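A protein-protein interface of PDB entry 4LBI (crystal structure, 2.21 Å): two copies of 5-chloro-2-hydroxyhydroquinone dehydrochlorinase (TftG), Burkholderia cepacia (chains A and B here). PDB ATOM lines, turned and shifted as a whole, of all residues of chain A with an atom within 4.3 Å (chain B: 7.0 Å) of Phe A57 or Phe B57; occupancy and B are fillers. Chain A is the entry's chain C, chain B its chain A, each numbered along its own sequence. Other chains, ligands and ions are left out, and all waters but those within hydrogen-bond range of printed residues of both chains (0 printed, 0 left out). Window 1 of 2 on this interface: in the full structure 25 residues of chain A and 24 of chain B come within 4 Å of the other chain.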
ATOM      1  N   LEU A   4      23.606  22.179  10.262  1.00  0.00           N
ATOM      2  CA  LEU A   4      24.413  23.065  11.082  1.00  0.00           C
ATOM      3  C   LEU A   4      24.901  24.156  10.154  1.00  0.00           C
ATOM      4  O   LEU A   4      25.366  23.872   9.059  1.00  0.00           O
ATOM      5  CB  LEU A   4      25.622  22.344  11.674  1.00  0.00           C
ATOM      6  CG  LEU A   4      25.397  21.042  12.436  1.00  0.00           C
ATOM      7  CD1 LEU A   4      26.702  20.574  13.023  1.00  0.00           C
ATOM      8  CD2 LEU A   4      24.334  21.210  13.527  1.00  0.00           C
ATOM      9  N   ILE A   5      24.779  25.403  10.585  1.00  0.00           N
ATOM     10  CA  ILE A   5      25.332  26.521   9.837  1.00  0.00           C
ATOM     11  C   ILE A   5      26.245  27.292  10.775  1.00  0.00           C
ATOM     12  O   ILE A   5      25.787  27.941  11.722  1.00  0.00           O
ATOM     13  CB  ILE A   5      24.234  27.436   9.259  1.00  0.00           C
ATOM     14  CG1 ILE A   5      23.190  26.592   8.536  1.00  0.00           C
ATOM     15  CG2 ILE A   5      24.835  28.488   8.315  1.00  0.00           C
ATOM     16  CD1 ILE A   5      22.155  27.390   7.836  1.00  0.00           C
ATOM     17  N   TYR A   6      27.542  27.202  10.496  1.00  0.00           N
ATOM     18  CA  TYR A   6      28.580  27.769  11.343  1.00  0.00           C
ATOM     19  C   TYR A   6      29.363  28.819  10.576  1.00  0.00           C
ATOM     20  O   TYR A   6      29.946  28.525   9.524  1.00  0.00           O
ATOM     21  CB  TYR A   6      29.528  26.652  11.786  1.00  0.00           C
ATOM     22  CG  TYR A   6      30.812  27.108  12.440  1.00  0.00           C
ATOM     23  CD1 TYR A   6      31.947  27.365  11.685  1.00  0.00           C
ATOM     24  CD2 TYR A   6      30.902  27.232  13.820  1.00  0.00           C
ATOM     25  CE1 TYR A   6      33.129  27.765  12.281  1.00  0.00           C
ATOM     26  CE2 TYR A   6      32.077  27.627  14.428  1.00  0.00           C
ATOM     27  CZ  TYR A   6      33.192  27.893  13.654  1.00  0.00           C
ATOM     28  OH  TYR A   6      34.366  28.288  14.262  1.00  0.00           O
ATOM     29  N   VAL A  37      17.943  26.065  16.764  1.00  0.00           N
ATOM     30  CA  VAL A  37      18.880  26.608  17.733  1.00  0.00           C
ATOM     31  C   VAL A  37      19.587  27.742  17.024  1.00  0.00           C
ATOM     32  O   VAL A  37      19.921  27.619  15.849  1.00  0.00           O
ATOM     33  CB  VAL A  37      19.946  25.557  18.158  1.00  0.00           C
ATOM     34  CG1 VAL A  37      20.994  26.189  19.072  1.00  0.00           C
ATOM     35  CG2 VAL A  37      19.303  24.355  18.839  1.00  0.00           C
ATOM     36  N   GLY A  38      19.815  28.848  17.725  1.00  0.00           N
ATOM     37  CA  GLY A  38      20.494  29.979  17.127  1.00  0.00           C
ATOM     38  C   GLY A  38      21.139  30.878  18.155  1.00  0.00           C
ATOM     39  O   GLY A  38      20.557  31.157  19.200  1.00  0.00           O
ATOM     40  N   GLY A  39      22.352  31.330  17.860  1.00  0.00           N
ATOM     41  CA  GLY A  39      23.023  32.296  18.706  1.00  0.00           C
ATOM     42  C   GLY A  39      24.422  32.607  18.224  1.00  0.00           C
ATOM     43  O   GLY A  39      24.993  31.873  17.421  1.00  0.00           O
ATOM     44  N   SER A  56      28.341  33.507  13.996  1.00  0.00           N
ATOM     45  CA  SER A  56      26.934  33.104  13.997  1.00  0.00           C
ATOM     46  C   SER A  56      26.764  31.599  13.843  1.00  0.00           C
ATOM     47  O   SER A  56      27.338  30.986  12.936  1.00  0.00           O
ATOM     48  CB  SER A  56      26.185  33.794  12.850  1.00  0.00           C
ATOM     49  OG  SER A  56      26.221  35.209  12.990  1.00  0.00           O
ATOM     50  N   PHE A  57      25.964  31.000  14.717  1.00  0.00           N
ATOM     51  CA  PHE A  57      25.649  29.582  14.581  1.00  0.00           C
ATOM     52  C   PHE A  57      24.143  29.348  14.540  1.00  0.00           C
ATOM     53  O   PHE A  57      23.383  30.000  15.259  1.00  0.00           O
ATOM     54  CB  PHE A  57      26.271  28.756  15.704  1.00  0.00           C
ATOM     55  CG  PHE A  57      25.926  27.303  15.626  1.00  0.00           C
ATOM     56  CD1 PHE A  57      26.579  26.472  14.727  1.00  0.00           C
ATOM     57  CD2 PHE A  57      24.920  26.775  16.415  1.00  0.00           C
ATOM     58  CE1 PHE A  57      26.253  25.135  14.633  1.00  0.00           C
ATOM     59  CE2 PHE A  57      24.584  25.451  16.326  1.00  0.00           C
ATOM     60  CZ  PHE A  57      25.255  24.622  15.428  1.00  0.00           C
ATOM     61  N   LEU A  58      23.716  28.411  13.701  1.00  0.00           N
ATOM     62  CA  LEU A  58      22.298  28.114  13.559  1.00  0.00           C
ATOM     63  C   LEU A  58      22.096  26.621  13.365  1.00  0.00           C
ATOM     64  O   LEU A  58      22.936  25.950  12.770  1.00  0.00           O
ATOM     65  CB  LEU A  58      21.735  28.824  12.328  1.00  0.00           C
ATOM     66  CG  LEU A  58      21.542  30.336  12.384  1.00  0.00           C
ATOM     67  CD1 LEU A  58      21.283  30.899  11.001  1.00  0.00           C
ATOM     68  CD2 LEU A  58      20.382  30.647  13.294  1.00  0.00           C
ATOM     69  N   ILE A  59      20.989  26.091  13.865  1.00  0.00           N
ATOM     70  CA  ILE A  59      20.531  24.797  13.397  1.00  0.00           C
ATOM     71  C   ILE A  59      19.205  25.014  12.692  1.00  0.00           C
ATOM     72  O   ILE A  59      18.227  25.467  13.295  1.00  0.00           O
ATOM     73  CB  ILE A  59      20.398  23.763  14.513  1.00  0.00           C
ATOM     74  CG1 ILE A  59      21.772  23.453  15.102  1.00  0.00           C
ATOM     75  CG2 ILE A  59      19.755  22.484  13.978  1.00  0.00           C
ATOM     76  CD1 ILE A  59      21.760  22.260  16.034  1.00  0.00           C
ATOM     77  N   TRP A  91      22.697  17.286   9.254  1.00  0.00           N
ATOM     78  CA  TRP A  91      22.739  16.890  10.660  1.00  0.00           C
ATOM     79  C   TRP A  91      21.416  16.277  11.147  1.00  0.00           C
ATOM     80  O   TRP A  91      20.371  16.442  10.509  1.00  0.00           O
ATOM     81  CB  TRP A  91      23.082  18.126  11.493  1.00  0.00           C
ATOM     82  CG  TRP A  91      23.204  17.914  12.968  1.00  0.00           C
ATOM     83  CD1 TRP A  91      24.288  17.430  13.639  1.00  0.00           C
ATOM     84  CD2 TRP A  91      22.219  18.220  13.965  1.00  0.00           C
ATOM     85  NE1 TRP A  91      24.033  17.394  14.990  1.00  0.00           N
ATOM     86  CE2 TRP A  91      22.776  17.884  15.218  1.00  0.00           C
ATOM     87  CE3 TRP A  91      20.923  18.745  13.919  1.00  0.00           C
ATOM     88  CZ2 TRP A  91      22.077  18.055  16.419  1.00  0.00           C
ATOM     89  CZ3 TRP A  91      20.231  18.911  15.108  1.00  0.00           C
ATOM     90  CH2 TRP A  91      20.811  18.567  16.345  1.00  0.00           C
ATOM     91  N   PHE B   3      29.295  25.824  25.164  1.00  0.00           N
ATOM     92  CA  PHE B   3      30.236  25.582  24.078  1.00  0.00           C
ATOM     93  C   PHE B   3      29.635  24.777  22.931  1.00  0.00           C
ATOM     94  O   PHE B   3      28.971  23.757  23.140  1.00  0.00           O
ATOM     95  CB  PHE B   3      31.488  24.855  24.583  1.00  0.00           C
ATOM     96  CG  PHE B   3      32.327  25.668  25.531  1.00  0.00           C
ATOM     97  CD1 PHE B   3      33.390  26.427  25.062  1.00  0.00           C
ATOM     98  CD2 PHE B   3      32.057  25.671  26.887  1.00  0.00           C
ATOM     99  CE1 PHE B   3      34.174  27.174  25.934  1.00  0.00           C
ATOM    100  CE2 PHE B   3      32.831  26.413  27.768  1.00  0.00           C
ATOM    101  CZ  PHE B   3      33.888  27.165  27.292  1.00  0.00           C
ATOM    102  N   LEU B   4      29.870  25.253  21.715  1.00  0.00           N
ATOM    103  CA  LEU B   4      29.724  24.426  20.530  1.00  0.00           C
ATOM    104  C   LEU B   4      30.916  23.470  20.477  1.00  0.00           C
ATOM    105  O   LEU B   4      32.061  23.901  20.609  1.00  0.00           O
ATOM    106  CB  LEU B   4      29.779  25.298  19.283  1.00  0.00           C
ATOM    107  CG  LEU B   4      28.832  26.484  19.149  1.00  0.00           C
ATOM    108  CD1 LEU B   4      28.951  27.041  17.735  1.00  0.00           C
ATOM    109  CD2 LEU B   4      27.396  26.069  19.460  1.00  0.00           C
ATOM    110  N   ILE B   5      30.662  22.180  20.282  1.00  0.00           N
ATOM    111  CA  ILE B   5      31.744  21.229  20.030  1.00  0.00           C
ATOM    112  C   ILE B   5      31.473  20.457  18.731  1.00  0.00           C
ATOM    113  O   ILE B   5      30.539  19.653  18.653  1.00  0.00           O
ATOM    114  CB  ILE B   5      31.948  20.246  21.209  1.00  0.00           C
ATOM    115  CG1 ILE B   5      32.058  21.011  22.533  1.00  0.00           C
ATOM    116  CG2 ILE B   5      33.199  19.397  20.984  1.00  0.00           C
ATOM    117  CD1 ILE B   5      32.007  20.124  23.760  1.00  0.00           C
ATOM    118  N   TYR B   6      32.301  20.725  17.725  1.00  0.00           N
ATOM    119  CA  TYR B   6      32.125  20.212  16.368  1.00  0.00           C
ATOM    120  C   TYR B   6      33.310  19.322  16.044  1.00  0.00           C
ATOM    121  O   TYR B   6      34.470  19.742  16.155  1.00  0.00           O
ATOM    122  CB  TYR B   6      32.020  21.393  15.392  1.00  0.00           C
ATOM    123  CG  TYR B   6      32.131  21.087  13.911  1.00  0.00           C
ATOM    124  CD1 TYR B   6      33.355  21.152  13.262  1.00  0.00           C
ATOM    125  CD2 TYR B   6      31.009  20.784  13.152  1.00  0.00           C
ATOM    126  CE1 TYR B   6      33.465  20.900  11.912  1.00  0.00           C
ATOM    127  CE2 TYR B   6      31.112  20.525  11.792  1.00  0.00           C
ATOM    128  CZ  TYR B   6      32.345  20.589  11.182  1.00  0.00           C
ATOM    129  OH  TYR B   6      32.473  20.342   9.834  1.00  0.00           O
ATOM    130  N   ARG B   7      33.019  18.085  15.655  1.00  0.00           N
ATOM    131  CA  ARG B   7      34.060  17.098  15.376  1.00  0.00           C
ATOM    132  C   ARG B   7      33.702  16.252  14.157  1.00  0.00           C
ATOM    133  O   ARG B   7      32.631  15.663  14.106  1.00  0.00           O
ATOM    134  CB  ARG B   7      34.297  16.202  16.604  1.00  0.00           C
ATOM    135  CG  ARG B   7      34.893  16.935  17.805  1.00  0.00           C
ATOM    136  CD  ARG B   7      34.933  16.064  19.056  1.00  0.00           C
ATOM    137  NE  ARG B   7      33.599  15.784  19.575  1.00  0.00           N
ATOM    138  CZ  ARG B   7      33.342  14.976  20.603  1.00  0.00           C
ATOM    139  NH1 ARG B   7      34.334  14.363  21.242  1.00  0.00           N
ATOM    140  NH2 ARG B   7      32.086  14.790  20.994  1.00  0.00           N
ATOM    141  N   ARG B  17      33.658   4.510  13.982  1.00  0.00           N
ATOM    142  CA  ARG B  17      32.454   5.093  14.587  1.00  0.00           C
ATOM    143  C   ARG B  17      31.431   4.029  15.017  1.00  0.00           C
ATOM    144  O   ARG B  17      30.971   4.040  16.159  1.00  0.00           O
ATOM    145  CB  ARG B  17      31.782   6.100  13.636  1.00  0.00           C
ATOM    146  CG  ARG B  17      30.376   6.552  14.085  1.00  0.00           C
ATOM    147  CD  ARG B  17      29.881   7.785  13.326  1.00  0.00           C
ATOM    148  NE  ARG B  17      30.646   8.962  13.704  1.00  0.00           N
ATOM    149  CZ  ARG B  17      30.322   9.805  14.681  1.00  0.00           C
ATOM    150  NH1 ARG B  17      29.208   9.652  15.379  1.00  0.00           N
ATOM    151  NH2 ARG B  17      31.120  10.821  14.951  1.00  0.00           N
ATOM    152  N   ILE B  35      24.349  18.687  28.507  1.00  0.00           N
ATOM    153  CA  ILE B  35      24.261  18.715  27.050  1.00  0.00           C
ATOM    154  C   ILE B  35      22.873  19.172  26.595  1.00  0.00           C
ATOM    155  O   ILE B  35      21.888  18.475  26.818  1.00  0.00           O
ATOM    156  CB  ILE B  35      24.517  17.320  26.468  1.00  0.00           C
ATOM    157  CG1 ILE B  35      25.913  16.832  26.859  1.00  0.00           C
ATOM    158  CG2 ILE B  35      24.300  17.322  24.957  1.00  0.00           C
ATOM    159  CD1 ILE B  35      26.175  15.415  26.488  1.00  0.00           C
ATOM    160  N   VAL B  37      22.046  20.191  23.248  1.00  0.00           N
ATOM    161  CA  VAL B  37      21.764  19.691  21.904  1.00  0.00           C
ATOM    162  C   VAL B  37      22.898  18.766  21.520  1.00  0.00           C
ATOM    163  O   VAL B  37      24.063  19.070  21.795  1.00  0.00           O
ATOM    164  CB  VAL B  37      21.737  20.832  20.867  1.00  0.00           C
ATOM    165  CG1 VAL B  37      21.574  20.282  19.459  1.00  0.00           C
ATOM    166  CG2 VAL B  37      20.633  21.796  21.177  1.00  0.00           C
ATOM    167  N   GLY B  38      22.560  17.647  20.878  1.00  0.00           N
ATOM    168  CA  GLY B  38      23.546  16.697  20.408  1.00  0.00           C
ATOM    169  C   GLY B  38      23.038  15.811  19.286  1.00  0.00           C
ATOM    170  O   GLY B  38      21.860  15.434  19.240  1.00  0.00           O
ATOM    171  N   GLY B  39      23.938  15.476  18.370  1.00  0.00           N
ATOM    172  CA  GLY B  39      23.623  14.557  17.294  1.00  0.00           C
ATOM    173  C   GLY B  39      24.744  14.565  16.287  1.00  0.00           C
ATOM    174  O   GLY B  39      25.605  15.441  16.331  1.00  0.00           O
ATOM    175  N   PRO B  40      24.740  13.592  15.368  1.00  0.00           N
ATOM    176  CA  PRO B  40      25.840  13.458  14.413  1.00  0.00           C
ATOM    177  C   PRO B  40      25.616  14.247  13.113  1.00  0.00           C
ATOM    178  O   PRO B  40      24.469  14.472  12.703  1.00  0.00           O
ATOM    179  CB  PRO B  40      25.828  11.966  14.110  1.00  0.00           C
ATOM    180  CG  PRO B  40      24.354  11.611  14.175  1.00  0.00           C
ATOM    181  CD  PRO B  40      23.746  12.511  15.226  1.00  0.00           C
ATOM    182  N   THR B  41      26.704  14.661  12.473  1.00  0.00           N
ATOM    183  CA  THR B  41      26.606  15.247  11.142  1.00  0.00           C
ATOM    184  C   THR B  41      26.391  14.085  10.191  1.00  0.00           C
ATOM    185  O   THR B  41      26.792  12.949  10.491  1.00  0.00           O
ATOM    186  CB  THR B  41      27.872  16.044  10.755  1.00  0.00           C
ATOM    187  OG1 THR B  41      29.020  15.190  10.822  1.00  0.00           O
ATOM    188  CG2 THR B  41      28.066  17.235  11.698  1.00  0.00           C
ATOM    189  N   GLY B  55      30.240  12.670  11.769  1.00  0.00           N
ATOM    190  CA  GLY B  55      30.830  13.483  12.817  1.00  0.00           C
ATOM    191  C   GLY B  55      29.901  13.640  14.004  1.00  0.00           C
ATOM    192  O   GLY B  55      28.836  13.029  14.043  1.00  0.00           O
ATOM    193  N   SER B  56      30.303  14.454  14.973  1.00  0.00           N
ATOM    194  CA  SER B  56      29.533  14.617  16.203  1.00  0.00           C
ATOM    195  C   SER B  56      29.431  16.086  16.543  1.00  0.00           C
ATOM    196  O   SER B  56      30.442  16.789  16.552  1.00  0.00           O
ATOM    197  CB  SER B  56      30.227  13.908  17.367  1.00  0.00           C
ATOM    198  OG  SER B  56      30.450  12.543  17.084  1.00  0.00           O
ATOM    199  N   PHE B  57      28.220  16.555  16.818  1.00  0.00           N
ATOM    200  CA  PHE B  57      28.045  17.932  17.260  1.00  0.00           C
ATOM    201  C   PHE B  57      27.401  17.983  18.633  1.00  0.00           C
ATOM    202  O   PHE B  57      26.486  17.202  18.920  1.00  0.00           O
ATOM    203  CB  PHE B  57      27.189  18.753  16.289  1.00  0.00           C
ATOM    204  CG  PHE B  57      26.954  20.158  16.766  1.00  0.00           C
ATOM    205  CD1 PHE B  57      27.976  21.111  16.691  1.00  0.00           C
ATOM    206  CD2 PHE B  57      25.735  20.526  17.327  1.00  0.00           C
ATOM    207  CE1 PHE B  57      27.771  22.421  17.150  1.00  0.00           C
ATOM    208  CE2 PHE B  57      25.522  21.821  17.788  1.00  0.00           C
ATOM    209  CZ  PHE B  57      26.544  22.764  17.708  1.00  0.00           C
ATOM    210  N   LEU B  58      27.860  18.914  19.468  1.00  0.00           N
ATOM    211  CA  LEU B  58      27.274  19.100  20.788  1.00  0.00           C
ATOM    212  C   LEU B  58      27.231  20.571  21.167  1.00  0.00           C
ATOM    213  O   LEU B  58      28.145  21.334  20.826  1.00  0.00           O
ATOM    214  CB  LEU B  58      28.112  18.396  21.849  1.00  0.00           C
ATOM    215  CG  LEU B  58      28.233  16.885  21.885  1.00  0.00           C
ATOM    216  CD1 LEU B  58      29.386  16.516  22.811  1.00  0.00           C
ATOM    217  CD2 LEU B  58      26.925  16.254  22.344  1.00  0.00           C
ATOM    218  N   ILE B  59      26.183  20.964  21.892  1.00  0.00           N
ATOM    219  CA  ILE B  59      26.234  22.194  22.668  1.00  0.00           C
ATOM    220  C   ILE B  59      26.230  21.811  24.129  1.00  0.00           C
ATOM    221  O   ILE B  59      25.298  21.167  24.615  1.00  0.00           O
ATOM    222  CB  ILE B  59      25.062  23.115  22.383  1.00  0.00           C
ATOM    223  CG1 ILE B  59      25.073  23.516  20.909  1.00  0.00           C
ATOM    224  CG2 ILE B  59      25.131  24.340  23.281  1.00  0.00           C
ATOM    225  CD1 ILE B  59      23.929  24.401  20.510  1.00  0.00           C
ATOM    226  N   ILE B  87      36.445  21.486  16.471  1.00  0.00           N
ATOM    227  CA  ILE B  87      36.265  22.929  16.638  1.00  0.00           C
ATOM    228  C   ILE B  87      35.397  23.180  17.862  1.00  0.00           C
ATOM    229  O   ILE B  87      34.319  22.598  17.999  1.00  0.00           O
ATOM    230  CB  ILE B  87      35.580  23.590  15.423  1.00  0.00           C
ATOM    231  CG1 ILE B  87      36.345  23.317  14.126  1.00  0.00           C
ATOM    232  CG2 ILE B  87      35.431  25.090  15.649  1.00  0.00           C
ATOM    233  CD1 ILE B  87      35.691  23.966  12.907  1.00  0.00           C
ATOM    234  N   TRP B  91      29.775  30.229  23.265  1.00  0.00           N
ATOM    235  CA  TRP B  91      28.535  30.491  22.530  1.00  0.00           C
ATOM    236  C   TRP B  91      27.394  30.845  23.475  1.00  0.00           C
ATOM    237  O   TRP B  91      27.461  30.563  24.680  1.00  0.00           O
ATOM    238  CB  TRP B  91      28.162  29.229  21.755  1.00  0.00           C
ATOM    239  CG  TRP B  91      26.924  29.329  20.945  1.00  0.00           C
ATOM    240  CD1 TRP B  91      26.798  29.886  19.700  1.00  0.00           C
ATOM    241  CD2 TRP B  91      25.627  28.841  21.299  1.00  0.00           C
ATOM    242  NE1 TRP B  91      25.501  29.782  19.264  1.00  0.00           N
ATOM    243  CE2 TRP B  91      24.760  29.142  20.225  1.00  0.00           C
ATOM    244  CE3 TRP B  91      25.110  28.182  22.418  1.00  0.00           C
ATOM    245  CZ2 TRP B  91      23.406  28.806  20.240  1.00  0.00           C
ATOM    246  CZ3 TRP B  91      23.761  27.844  22.429  1.00  0.00           C
ATOM    247  CH2 TRP B  91      22.926  28.156  21.347  1.00  0.00           C
ATOM    248  N   LYS B  92      26.346  31.456  22.937  1.00  0.00           N
ATOM    249  CA  LYS B  92      25.142  31.726  23.721  1.00  0.00           C
ATOM    250  C   LYS B  92      23.930  31.731  22.810  1.00  0.00           C
ATOM    251  O   LYS B  92      24.057  32.023  21.615  1.00  0.00           O
ATOM    252  CB  LYS B  92      25.243  33.075  24.443  1.00  0.00           C
ATOM    253  CG  LYS B  92      25.093  34.278  23.540  1.00  0.00           C
ATOM    254  CD  LYS B  92      24.742  35.531  24.337  1.00  0.00           C
ATOM    255  CE  LYS B  92      24.503  36.714  23.408  1.00  0.00           C
ATOM    256  NZ  LYS B  92      24.135  37.964  24.135  1.00  0.00           N
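O of Gly B39 sits at hydrogen-bond distance from NE1 of Trp A91, at 2.8 Å. The indole nitrogen (NE1) of Trp B91 lies within hydrogen-bond range of the backbone carbonyl oxygen (O) of Gly A39 (2.8 Å).
O of Gly A39 sits at hydrogen-bond distance from N of Phe A57. The backbone NH (N) of Gly B55 lies within hydrogen-bond range of the side-chain hydroxyl (OG1) of Thr B41 (3.0 Å). N of Ile A59 is in hydrogen-bond range of O of Val A37 (2.7 Å). O of Val B37 sits at hydrogen-bond distance from N of Ile B59. O of Tyr B6 lies within hydrogen-bond range of N of Ile B87 (2.7 Å). The backbone carbonyl oxygen of Gly B39 lies within hydrogen-bond range of the backbone NH of Phe B57.
Among the printed residues, pairs that only touch across the chains: Gly A39 with Lys B92 (3.1 Å), Trp A91 with Pro B40 (3.1 Å), Phe A57 with Phe B57 (3.2 Å), Val A37 with Trp B91 (3.6 Å), Trp A91 with Val B37 (3.6 Å), Tyr A6 with Ile B87 (3.6 Å), Trp A91 with Phe B57 (3.7 Å), Phe A57 with Leu B4 (3.7 Å), Gly A38 with Trp B91 (3.7 Å), Val A37 with Val B37 (3.7 Å), Val A37 with Ile B59 (3.7 Å), Trp A91 with Gly B38 (3.8 Å), Leu A4 with Phe B57 (3.8 Å), Phe A57 with Trp B91 (3.8 Å), Leu A4 with Thr B41 (3.8 Å), Trp A91 with Thr B41 (3.9 Å) and Ile A59 with Val B37 (3.96 Å).
Phe A57 touches three residues of chain B. Of the printed residues of chain A, Thr B41 touches Leu A4 and Trp A91. Printed residues of chain A within 4 Å of Gly B39: Trp A91 (2.8 Å). Printed residues of chain A within 4 Å of Ile B87: Tyr A6. Of the printed residues of chain B, Tyr A6 touches Ile B87 (3.6 Å). Leu B58 touches none of the printed residues of chain A. The nearest printed residue of chain B that does not touch Val A37 is Leu B4 (6.4 Å).
Printed residues of chain B that touch a printed residue of chain A: Leu B4, Val B37, Gly B38, Gly B39, Pro B40, Thr B41, Phe B57, Ile B59, Ile B87, Trp B91 and Lys B92. Hydrophobic or aromatic side chains of chain B within 4 Å of the printed part of chain A: Leu B4, Val B37, Phe B57, Ile B59, Ile B87 and Trp B91. Of the 11 printed residues of chain A, 8 touch a printed residue of chain B. Among the printed residues, no Asp or Glu carboxylate lies within 4 Å of a Lys or Arg side-chain nitrogen of the other chain.
Leu A4 touches Phe B57, and with the chains exchanged Phe A57 touches Leu B4. Val A37 touches Trp B91, and with the chains exchanged Trp A91 touches Val B37. Gly A38 touches Trp B91, and with the chains exchanged Trp A91 touches Gly B38. Phe A57 touches its own counterpart, Phe B57.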
